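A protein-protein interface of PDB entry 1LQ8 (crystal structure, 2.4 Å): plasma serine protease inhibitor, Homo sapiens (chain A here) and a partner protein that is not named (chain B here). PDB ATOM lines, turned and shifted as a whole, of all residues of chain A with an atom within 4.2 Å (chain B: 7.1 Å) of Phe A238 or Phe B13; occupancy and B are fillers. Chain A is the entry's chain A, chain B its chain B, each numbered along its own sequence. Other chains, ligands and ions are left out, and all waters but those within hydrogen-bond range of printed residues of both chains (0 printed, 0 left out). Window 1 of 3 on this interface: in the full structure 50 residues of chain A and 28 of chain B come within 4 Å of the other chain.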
ATOM      1  N   TRP A 180     -40.069 -13.991  -8.371  1.00  0.00           N
ATOM      2  CA  TRP A 180     -38.833 -13.709  -7.656  1.00  0.00           C
ATOM      3  C   TRP A 180     -39.148 -13.614  -6.173  1.00  0.00           C
ATOM      4  O   TRP A 180     -40.298 -13.373  -5.800  1.00  0.00           O
ATOM      5  CB  TRP A 180     -38.254 -12.374  -8.102  1.00  0.00           C
ATOM      6  CG  TRP A 180     -37.803 -12.365  -9.497  1.00  0.00           C
ATOM      7  CD1 TRP A 180     -38.324 -11.633 -10.523  1.00  0.00           C
ATOM      8  CD2 TRP A 180     -36.708 -13.103 -10.036  1.00  0.00           C
ATOM      9  NE1 TRP A 180     -37.618 -11.870 -11.674  1.00  0.00           N
ATOM     10  CE2 TRP A 180     -36.618 -12.768 -11.406  1.00  0.00           C
ATOM     11  CE3 TRP A 180     -35.791 -14.013  -9.496  1.00  0.00           C
ATOM     12  CZ2 TRP A 180     -35.642 -13.310 -12.246  1.00  0.00           C
ATOM     13  CZ3 TRP A 180     -34.819 -14.554 -10.329  1.00  0.00           C
ATOM     14  CH2 TRP A 180     -34.753 -14.200 -11.691  1.00  0.00           C
ATOM     15  N   PHE A 194     -27.787  -1.822 -24.652  1.00  0.00           N
ATOM     16  CA  PHE A 194     -27.175  -3.124 -24.424  1.00  0.00           C
ATOM     17  C   PHE A 194     -26.155  -3.353 -25.529  1.00  0.00           C
ATOM     18  O   PHE A 194     -26.479  -3.315 -26.728  1.00  0.00           O
ATOM     19  CB  PHE A 194     -28.239  -4.222 -24.433  1.00  0.00           C
ATOM     20  CG  PHE A 194     -27.715  -5.579 -24.045  1.00  0.00           C
ATOM     21  CD1 PHE A 194     -27.072  -6.392 -24.985  1.00  0.00           C
ATOM     22  CD2 PHE A 194     -27.879  -6.054 -22.738  1.00  0.00           C
ATOM     23  CE1 PHE A 194     -26.609  -7.654 -24.628  1.00  0.00           C
ATOM     24  CE2 PHE A 194     -27.419  -7.315 -22.369  1.00  0.00           C
ATOM     25  CZ  PHE A 194     -26.784  -8.121 -23.310  1.00  0.00           C
ATOM     26  N   ARG A 224     -18.272 -11.359 -12.682  1.00  0.00           N
ATOM     27  CA  ARG A 224     -19.014 -11.084 -11.458  1.00  0.00           C
ATOM     28  C   ARG A 224     -20.305 -11.906 -11.467  1.00  0.00           C
ATOM     29  O   ARG A 224     -21.007 -11.985 -12.484  1.00  0.00           O
ATOM     30  CB  ARG A 224     -19.326  -9.591 -11.355  1.00  0.00           C
ATOM     31  CG  ARG A 224     -18.082  -8.712 -11.190  1.00  0.00           C
ATOM     32  CD  ARG A 224     -18.441  -7.248 -11.124  1.00  0.00           C
ATOM     33  NE  ARG A 224     -17.294  -6.412 -10.795  1.00  0.00           N
ATOM     34  CZ  ARG A 224     -16.288  -6.130 -11.620  1.00  0.00           C
ATOM     35  NH1 ARG A 224     -15.300  -5.354 -11.198  1.00  0.00           N
ATOM     36  NH2 ARG A 224     -16.261  -6.608 -12.859  1.00  0.00           N
ATOM     37  N   VAL A 225     -20.615 -12.530 -10.335  1.00  0.00           N
ATOM     38  CA  VAL A 225     -21.803 -13.365 -10.247  1.00  0.00           C
ATOM     39  C   VAL A 225     -22.796 -12.896  -9.188  1.00  0.00           C
ATOM     40  O   VAL A 225     -22.429 -12.616  -8.045  1.00  0.00           O
ATOM     41  CB  VAL A 225     -21.427 -14.835  -9.958  1.00  0.00           C
ATOM     42  CG1 VAL A 225     -22.609 -15.731 -10.257  1.00  0.00           C
ATOM     43  CG2 VAL A 225     -20.219 -15.249 -10.793  1.00  0.00           C
ATOM     44  N   VAL A 226     -24.061 -12.817  -9.590  1.00  0.00           N
ATOM     45  CA  VAL A 226     -25.142 -12.398  -8.709  1.00  0.00           C
ATOM     46  C   VAL A 226     -26.126 -13.535  -8.532  1.00  0.00           C
ATOM     47  O   VAL A 226     -26.456 -14.243  -9.489  1.00  0.00           O
ATOM     48  CB  VAL A 226     -25.955 -11.243  -9.299  1.00  0.00           C
ATOM     49  CG1 VAL A 226     -26.014 -10.112  -8.320  1.00  0.00           C
ATOM     50  CG2 VAL A 226     -25.369 -10.810 -10.635  1.00  0.00           C
ATOM     51  N   ALA A 236     -31.519 -18.005  -9.440  1.00  0.00           N
ATOM     52  CA  ALA A 236     -31.000 -17.704 -10.742  1.00  0.00           C
ATOM     53  C   ALA A 236     -29.595 -17.146 -10.515  1.00  0.00           C
ATOM     54  O   ALA A 236     -29.381 -16.322  -9.620  1.00  0.00           O
ATOM     55  CB  ALA A 236     -31.873 -16.673 -11.423  1.00  0.00           C
ATOM     56  N   LEU A 237     -28.627 -17.614 -11.291  1.00  0.00           N
ATOM     57  CA  LEU A 237     -27.277 -17.094 -11.182  1.00  0.00           C
ATOM     58  C   LEU A 237     -27.019 -16.365 -12.495  1.00  0.00           C
ATOM     59  O   LEU A 237     -27.155 -16.951 -13.569  1.00  0.00           O
ATOM     60  CB  LEU A 237     -26.266 -18.227 -10.996  1.00  0.00           C
ATOM     61  CG  LEU A 237     -26.479 -19.164  -9.803  1.00  0.00           C
ATOM     62  CD1 LEU A 237     -25.396 -20.248  -9.817  1.00  0.00           C
ATOM     63  CD2 LEU A 237     -26.448 -18.384  -8.499  1.00  0.00           C
ATOM     64  N   PHE A 238     -26.688 -15.081 -12.417  1.00  0.00           N
ATOM     65  CA  PHE A 238     -26.403 -14.290 -13.612  1.00  0.00           C
ATOM     66  C   PHE A 238     -24.905 -13.971 -13.624  1.00  0.00           C
ATOM     67  O   PHE A 238     -24.406 -13.275 -12.742  1.00  0.00           O
ATOM     68  CB  PHE A 238     -27.227 -12.989 -13.610  1.00  0.00           C
ATOM     69  CG  PHE A 238     -28.702 -13.193 -13.851  1.00  0.00           C
ATOM     70  CD1 PHE A 238     -29.631 -12.945 -12.845  1.00  0.00           C
ATOM     71  CD2 PHE A 238     -29.166 -13.647 -15.084  1.00  0.00           C
ATOM     72  CE1 PHE A 238     -31.003 -13.142 -13.060  1.00  0.00           C
ATOM     73  CE2 PHE A 238     -30.544 -13.848 -15.313  1.00  0.00           C
ATOM     74  CZ  PHE A 238     -31.460 -13.599 -14.300  1.00  0.00           C
ATOM     75  N   ILE A 239     -24.188 -14.491 -14.612  1.00  0.00           N
ATOM     76  CA  ILE A 239     -22.752 -14.258 -14.705  1.00  0.00           C
ATOM     77  C   ILE A 239     -22.383 -13.134 -15.690  1.00  0.00           C
ATOM     78  O   ILE A 239     -22.706 -13.192 -16.883  1.00  0.00           O
ATOM     79  CB  ILE A 239     -21.997 -15.548 -15.131  1.00  0.00           C
ATOM     80  CG1 ILE A 239     -22.042 -16.590 -14.010  1.00  0.00           C
ATOM     81  CG2 ILE A 239     -20.533 -15.225 -15.444  1.00  0.00           C
ATOM     82  CD1 ILE A 239     -23.401 -17.185 -13.734  1.00  0.00           C
ATOM     83  N   LEU A 240     -21.707 -12.108 -15.185  1.00  0.00           N
ATOM     84  CA  LEU A 240     -21.285 -11.015 -16.047  1.00  0.00           C
ATOM     85  C   LEU A 240     -19.771 -11.044 -16.190  1.00  0.00           C
ATOM     86  O   LEU A 240     -19.047 -10.614 -15.295  1.00  0.00           O
ATOM     87  CB  LEU A 240     -21.723  -9.660 -15.485  1.00  0.00           C
ATOM     88  CG  LEU A 240     -21.124  -8.474 -16.254  1.00  0.00           C
ATOM     89  CD1 LEU A 240     -21.627  -8.482 -17.691  1.00  0.00           C
ATOM     90  CD2 LEU A 240     -21.490  -7.165 -15.569  1.00  0.00           C
ATOM     91  N   MET A 246     -15.846 -12.961 -21.962  1.00  0.00           N
ATOM     92  CA  MET A 246     -16.876 -13.992 -22.069  1.00  0.00           C
ATOM     93  C   MET A 246     -16.256 -15.359 -22.424  1.00  0.00           C
ATOM     94  O   MET A 246     -16.465 -16.350 -21.716  1.00  0.00           O
ATOM     95  CB  MET A 246     -17.906 -13.597 -23.127  1.00  0.00           C
ATOM     96  CG  MET A 246     -18.925 -14.689 -23.451  1.00  0.00           C
ATOM     97  SD  MET A 246     -19.782 -15.330 -21.991  1.00  0.00           S
ATOM     98  CE  MET A 246     -21.295 -14.315 -21.988  1.00  0.00           C
ATOM     99  N   LEU A 274     -30.819  -5.492 -14.573  1.00  0.00           N
ATOM    100  CA  LEU A 274     -30.940  -6.713 -15.364  1.00  0.00           C
ATOM    101  C   LEU A 274     -31.876  -6.534 -16.553  1.00  0.00           C
ATOM    102  O   LEU A 274     -32.982  -6.011 -16.431  1.00  0.00           O
ATOM    103  CB  LEU A 274     -31.449  -7.843 -14.464  1.00  0.00           C
ATOM    104  CG  LEU A 274     -31.435  -9.288 -14.954  1.00  0.00           C
ATOM    105  CD1 LEU A 274     -30.013  -9.749 -15.153  1.00  0.00           C
ATOM    106  CD2 LEU A 274     -32.120 -10.164 -13.930  1.00  0.00           C
ATOM    107  N   PRO A 275     -31.445  -6.971 -17.732  1.00  0.00           N
ATOM    108  CA  PRO A 275     -32.419  -6.745 -18.792  1.00  0.00           C
ATOM    109  C   PRO A 275     -33.545  -7.759 -18.788  1.00  0.00           C
ATOM    110  O   PRO A 275     -33.335  -8.930 -18.483  1.00  0.00           O
ATOM    111  CB  PRO A 275     -31.567  -6.793 -20.060  1.00  0.00           C
ATOM    112  CG  PRO A 275     -30.452  -7.709 -19.695  1.00  0.00           C
ATOM    113  CD  PRO A 275     -30.126  -7.342 -18.271  1.00  0.00           C
ATOM    114  N   PHE A 277     -35.670 -10.191 -20.524  1.00  0.00           N
ATOM    115  CA  PHE A 277     -35.363 -10.884 -21.758  1.00  0.00           C
ATOM    116  C   PHE A 277     -36.085 -12.194 -21.950  1.00  0.00           C
ATOM    117  O   PHE A 277     -36.776 -12.702 -21.056  1.00  0.00           O
ATOM    118  CB  PHE A 277     -33.859 -11.140 -21.833  1.00  0.00           C
ATOM    119  CG  PHE A 277     -33.367 -12.124 -20.810  1.00  0.00           C
ATOM    120  CD1 PHE A 277     -33.193 -13.466 -21.140  1.00  0.00           C
ATOM    121  CD2 PHE A 277     -33.118 -11.721 -19.496  1.00  0.00           C
ATOM    122  CE1 PHE A 277     -32.774 -14.391 -20.175  1.00  0.00           C
ATOM    123  CE2 PHE A 277     -32.700 -12.640 -18.522  1.00  0.00           C
ATOM    124  CZ  PHE A 277     -32.528 -13.975 -18.863  1.00  0.00           C
ATOM    125  N   LEU B   7     -24.217  -2.861 -10.489  1.00  0.00           N
ATOM    126  CA  LEU B   7     -24.020  -4.045 -11.321  1.00  0.00           C
ATOM    127  C   LEU B   7     -25.060  -4.023 -12.443  1.00  0.00           C
ATOM    128  O   LEU B   7     -26.241  -4.304 -12.222  1.00  0.00           O
ATOM    129  CB  LEU B   7     -24.138  -5.342 -10.499  1.00  0.00           C
ATOM    130  CG  LEU B   7     -23.897  -6.644 -11.295  1.00  0.00           C
ATOM    131  CD1 LEU B   7     -22.605  -6.516 -12.095  1.00  0.00           C
ATOM    132  CD2 LEU B   7     -23.864  -7.853 -10.368  1.00  0.00           C
ATOM    133  N   PHE B   9     -26.072  -5.494 -16.142  1.00  0.00           N
ATOM    134  CA  PHE B   9     -25.885  -6.487 -17.183  1.00  0.00           C
ATOM    135  C   PHE B   9     -26.217  -5.902 -18.540  1.00  0.00           C
ATOM    136  O   PHE B   9     -27.322  -6.079 -19.034  1.00  0.00           O
ATOM    137  CB  PHE B   9     -26.756  -7.723 -16.911  1.00  0.00           C
ATOM    138  CG  PHE B   9     -26.214  -8.617 -15.828  1.00  0.00           C
ATOM    139  CD1 PHE B   9     -26.185  -8.191 -14.500  1.00  0.00           C
ATOM    140  CD2 PHE B   9     -25.659  -9.852 -16.140  1.00  0.00           C
ATOM    141  CE1 PHE B   9     -25.601  -8.983 -13.503  1.00  0.00           C
ATOM    142  CE2 PHE B   9     -25.071 -10.651 -15.144  1.00  0.00           C
ATOM    143  CZ  PHE B   9     -25.041 -10.210 -13.827  1.00  0.00           C
ATOM    144  N   ASN B  10     -25.264  -5.194 -19.141  1.00  0.00           N
ATOM    145  CA  ASN B  10     -25.508  -4.617 -20.458  1.00  0.00           C
ATOM    146  C   ASN B  10     -24.609  -5.204 -21.533  1.00  0.00           C
ATOM    147  O   ASN B  10     -24.368  -4.575 -22.555  1.00  0.00           O
ATOM    148  CB  ASN B  10     -25.365  -3.088 -20.434  1.00  0.00           C
ATOM    149  CG  ASN B  10     -24.018  -2.624 -19.915  1.00  0.00           C
ATOM    150  OD1 ASN B  10     -23.134  -3.428 -19.621  1.00  0.00           O
ATOM    151  ND2 ASN B  10     -23.857  -1.310 -19.801  1.00  0.00           N
ATOM    152  N   ARG B  11     -24.104  -6.407 -21.291  1.00  0.00           N
ATOM    153  CA  ARG B  11     -23.254  -7.108 -22.252  1.00  0.00           C
ATOM    154  C   ARG B  11     -23.643  -8.583 -22.130  1.00  0.00           C
ATOM    155  O   ARG B  11     -24.227  -8.996 -21.120  1.00  0.00           O
ATOM    156  CB  ARG B  11     -21.753  -6.982 -21.914  1.00  0.00           C
ATOM    157  CG  ARG B  11     -21.187  -5.588 -21.778  1.00  0.00           C
ATOM    158  CD  ARG B  11     -19.658  -5.641 -21.662  1.00  0.00           C
ATOM    159  NE  ARG B  11     -19.176  -6.239 -20.416  1.00  0.00           N
ATOM    160  CZ  ARG B  11     -19.201  -5.631 -19.231  1.00  0.00           C
ATOM    161  NH1 ARG B  11     -18.744  -6.248 -18.152  1.00  0.00           N
ATOM    162  NH2 ARG B  11     -19.687  -4.405 -19.119  1.00  0.00           N
ATOM    163  N   PRO B  12     -23.316  -9.397 -23.150  1.00  0.00           N
ATOM    164  CA  PRO B  12     -23.655 -10.819 -23.099  1.00  0.00           C
ATOM    165  C   PRO B  12     -23.436 -11.334 -21.682  1.00  0.00           C
ATOM    166  O   PRO B  12     -22.550 -10.858 -20.990  1.00  0.00           O
ATOM    167  CB  PRO B  12     -22.680 -11.422 -24.094  1.00  0.00           C
ATOM    168  CG  PRO B  12     -22.607 -10.357 -25.149  1.00  0.00           C
ATOM    169  CD  PRO B  12     -22.479  -9.095 -24.326  1.00  0.00           C
ATOM    170  N   PHE B  13     -24.252 -12.282 -21.240  1.00  0.00           N
ATOM    171  CA  PHE B  13     -24.096 -12.827 -19.897  1.00  0.00           C
ATOM    172  C   PHE B  13     -24.737 -14.205 -19.776  1.00  0.00           C
ATOM    173  O   PHE B  13     -25.751 -14.484 -20.406  1.00  0.00           O
ATOM    174  CB  PHE B  13     -24.711 -11.884 -18.851  1.00  0.00           C
ATOM    175  CG  PHE B  13     -26.190 -11.668 -19.021  1.00  0.00           C
ATOM    176  CD1 PHE B  13     -26.668 -10.723 -19.921  1.00  0.00           C
ATOM    177  CD2 PHE B  13     -27.105 -12.439 -18.309  1.00  0.00           C
ATOM    178  CE1 PHE B  13     -28.043 -10.547 -20.117  1.00  0.00           C
ATOM    179  CE2 PHE B  13     -28.485 -12.279 -18.491  1.00  0.00           C
ATOM    180  CZ  PHE B  13     -28.955 -11.332 -19.398  1.00  0.00           C
ATOM    181  N   LEU B  14     -24.133 -15.063 -18.966  1.00  0.00           N
ATOM    182  CA  LEU B  14     -24.636 -16.411 -18.742  1.00  0.00           C
ATOM    183  C   LEU B  14     -25.801 -16.396 -17.770  1.00  0.00           C
ATOM    184  O   LEU B  14     -26.000 -15.434 -17.033  1.00  0.00           O
ATOM    185  CB  LEU B  14     -23.546 -17.286 -18.141  1.00  0.00           C
ATOM    186  CG  LEU B  14     -22.589 -18.023 -19.070  1.00  0.00           C
ATOM    187  CD1 LEU B  14     -22.105 -17.144 -20.227  1.00  0.00           C
ATOM    188  CD2 LEU B  14     -21.445 -18.520 -18.210  1.00  0.00           C
ATOM    189  N   MET B  15     -26.572 -17.470 -17.770  1.00  0.00           N
ATOM    190  CA  MET B  15     -27.670 -17.586 -16.840  1.00  0.00           C
ATOM    191  C   MET B  15     -27.767 -19.023 -16.380  1.00  0.00           C
ATOM    192  O   MET B  15     -27.651 -19.939 -17.185  1.00  0.00           O
ATOM    193  CB  MET B  15     -28.995 -17.191 -17.469  1.00  0.00           C
ATOM    194  CG  MET B  15     -30.052 -17.043 -16.413  1.00  0.00           C
ATOM    195  SD  MET B  15     -31.714 -17.281 -16.970  1.00  0.00           S
ATOM    196  CE  MET B  15     -32.639 -16.962 -15.436  1.00  0.00           C
ATOM    197  N   PHE B  16     -27.953 -19.207 -15.075  1.00  0.00           N
ATOM    198  CA  PHE B  16     -28.102 -20.532 -14.473  1.00  0.00           C
ATOM    199  C   PHE B  16     -29.412 -20.517 -13.713  1.00  0.00           C
ATOM    200  O   PHE B  16     -29.733 -19.519 -13.079  1.00  0.00           O
ATOM    201  CB  PHE B  16     -27.058 -20.800 -13.397  1.00  0.00           C
ATOM    202  CG  PHE B  16     -25.730 -21.245 -13.897  1.00  0.00           C
ATOM    203  CD1 PHE B  16     -24.949 -20.420 -14.690  1.00  0.00           C
ATOM    204  CD2 PHE B  16     -25.206 -22.454 -13.459  1.00  0.00           C
ATOM    205  CE1 PHE B  16     -23.661 -20.791 -15.032  1.00  0.00           C
ATOM    206  CE2 PHE B  16     -23.922 -22.832 -13.796  1.00  0.00           C
ATOM    207  CZ  PHE B  16     -23.145 -21.994 -14.583  1.00  0.00           C
ATOM    208  N   GLY B  26     -27.741 -21.101 -20.076  1.00  0.00           N
ATOM    209  CA  GLY B  26     -27.716 -20.462 -21.375  1.00  0.00           C
ATOM    210  C   GLY B  26     -26.907 -19.178 -21.376  1.00  0.00           C
ATOM    211  O   GLY B  26     -26.456 -18.690 -20.323  1.00  0.00           O
ATOM    212  N   LYS B  27     -26.712 -18.626 -22.567  1.00  0.00           N
ATOM    213  CA  LYS B  27     -25.996 -17.376 -22.717  1.00  0.00           C
ATOM    214  C   LYS B  27     -26.960 -16.382 -23.353  1.00  0.00           C
ATOM    215  O   LYS B  27     -27.629 -16.708 -24.337  1.00  0.00           O
ATOM    216  CB  LYS B  27     -24.786 -17.562 -23.628  1.00  0.00           C
ATOM    217  CG  LYS B  27     -23.896 -16.333 -23.744  1.00  0.00           C
ATOM    218  CD  LYS B  27     -23.047 -16.317 -25.033  1.00  0.00           C
ATOM    219  CE  LYS B  27     -22.235 -17.585 -25.224  1.00  0.00           C
ATOM    220  NZ  LYS B  27     -21.283 -17.476 -26.365  1.00  0.00           N
ATOM    221  N   VAL B  28     -27.071 -15.190 -22.772  1.00  0.00           N
ATOM    222  CA  VAL B  28     -27.917 -14.150 -23.332  1.00  0.00           C
ATOM    223  C   VAL B  28     -26.929 -13.273 -24.067  1.00  0.00           C
ATOM    224  O   VAL B  28     -26.220 -12.449 -23.466  1.00  0.00           O
ATOM    225  CB  VAL B  28     -28.622 -13.309 -22.265  1.00  0.00           C
ATOM    226  CG1 VAL B  28     -29.361 -12.155 -22.938  1.00  0.00           C
ATOM    227  CG2 VAL B  28     -29.596 -14.159 -21.494  1.00  0.00           C
ATOM    228  N   ASN B  29     -26.859 -13.487 -25.374  1.00  0.00           N
ATOM    229  CA  ASN B  29     -25.944 -12.760 -26.229  1.00  0.00           C
ATOM    230  C   ASN B  29     -26.592 -11.502 -26.743  1.00  0.00           C
ATOM    231  O   ASN B  29     -25.917 -10.530 -27.064  1.00  0.00           O
ATOM    232  CB  ASN B  29     -25.515 -13.648 -27.400  1.00  0.00           C
ATOM    233  CG  ASN B  29     -24.603 -12.929 -28.370  1.00  0.00           C
ATOM    234  OD1 ASN B  29     -25.061 -12.338 -29.355  1.00  0.00           O
ATOM    235  ND2 ASN B  29     -23.301 -12.957 -28.085  1.00  0.00           N
ATOM    236  N   ARG B  30     -27.915 -11.522 -26.793  1.00  0.00           N
ATOM    237  CA  ARG B  30     -28.681 -10.394 -27.291  1.00  0.00           C
ATOM    238  C   ARG B  30     -30.138 -10.511 -26.866  1.00  0.00           C
ATOM    239  O   ARG B  30     -30.857 -11.361 -27.369  1.00  0.00           O
ATOM    240  CB  ARG B  30     -28.583 -10.373 -28.814  1.00  0.00           C
ATOM    241  CG  ARG B  30     -29.494  -9.393 -29.485  1.00  0.00           C
ATOM    242  CD  ARG B  30     -29.010  -9.110 -30.887  1.00  0.00           C
ATOM    243  NE  ARG B  30     -29.781  -8.037 -31.500  1.00  0.00           N
ATOM    244  CZ  ARG B  30     -29.386  -7.359 -32.567  1.00  0.00           C
ATOM    245  NH1 ARG B  30     -30.158  -6.394 -33.057  1.00  0.00           N
ATOM    246  NH2 ARG B  30     -28.217  -7.639 -33.137  1.00  0.00           N
ATOM    247  N   PRO B  31     -30.591  -9.659 -25.927  1.00  0.00           N
ATOM    248  CA  PRO B  31     -31.981  -9.725 -25.484  1.00  0.00           C
ATOM    249  C   PRO B  31     -32.922  -9.814 -26.678  1.00  0.00           C
ATOM    250  O   PRO B  31     -33.814 -10.688 -26.646  1.00  0.00           O
ATOM    251  CB  PRO B  31     -32.152  -8.432 -24.694  1.00  0.00           C
ATOM    252  CG  PRO B  31     -30.810  -8.245 -24.077  1.00  0.00           C
ATOM    253  CD  PRO B  31     -29.872  -8.577 -25.227  1.00  0.00           C
ATOM    254  OXT PRO B  31     -32.751  -9.018 -27.628  1.00  0.00           O
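The backbone NH of Phe B16 sits at hydrogen-bond distance from the backbone carbonyl oxygen of Leu A237.
N of Leu B14 is in hydrogen-bond range of O of Ile A239, 3.1 Å away.
The backbone carbonyl oxygen (O) of Phe B13 sits at hydrogen-bond distance from the backbone NH (N) of Val B28, 2.8 Å away.
N of Met B15 sits at hydrogen-bond distance from O of Gly B26 (2.8 Å).
The backbone carbonyl oxygen of Arg A224 is in hydrogen-bond range of the backbone NH of Leu A240, 2.8 Å away.
The backbone carbonyl oxygen (O) of Val A226 is in hydrogen-bond range of the backbone NH (N) of Phe A238 (3.1 Å).
Among the printed residues, merely in contact across the chains: Ile A239 with Phe B13, Pro A275 with Phe B9, Ala A236 with Phe B16, Val A226 with Phe B9, Phe A238 with Phe B9, Val A226 with Leu B7, Leu A237 with Met B15, Phe A194 with Arg B11, Phe A238 with Met B15, Met A246 with Leu B14, Phe A194 with Pro B31, Phe A277 with Val B28, Leu A240 with Phe B9, Phe A194 with Phe B9, Phe A194 with Asn B10, Phe A238 with Leu B14, Met A246 with Phe B13, Leu A240 with Arg B11, Met A246 with Pro B12, Phe A194 with Pro B12, Ile A239 with Phe B9, Leu A240 with Leu B7, Ile A239 with Phe B16, Met A246 with Lys B27, Phe A238 with Phe B13, Pro A275 with Phe B13, Phe A194 with Asn B29, Phe A277 with Met B15, Leu A237 with Leu B14 and Phe A194 with Phe B13.
Of the printed residues of chain B, Phe A194 touches Phe B9 (3.6 Å), Asn B10 (3.6 Å), Arg B11 (3.4 Å), Pro B12 (3.7 Å), Phe B13 (3.99 Å), Asn B29 (3.8 Å) and Pro B31 (3.4 Å).
Arg A224 touches none of the printed residues of chain B.
Printed residues of chain B within 4 Å of Val A226: Leu B7 (3.3 Å) and Phe B9 (3.3 Å).
Of the printed residues of chain B, Phe A238 touches Phe B9, Phe B13, Leu B14 and Met B15.
Printed residues of chain B within 4 Å of Phe A277: Met B15 (3.9 Å) and Val B28 (3.4 Å).
Printed residues of chain A within 4 Å of Phe B13: Phe A194 (3.99 Å), Phe A238 (3.7 Å), Ile A239 (3.1 Å), Met A246 (3.7 Å) and Pro A275 (3.7 Å).
Printed residues of chain A within 4 Å of Lys B27: Met A246.
The nearest residue of chain B that does not touch Phe A238 is Phe B16 (5.1 Å).
Hydrophobic or aromatic side chains of chain B that line the printed part of chain A: Leu B7, Phe B9, Pro B12, Phe B13, Leu B14, Met B15, Phe B16, Val B28 and Pro B31.
Of the 14 printed residues of chain A, 10 touch a printed residue of chain B.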
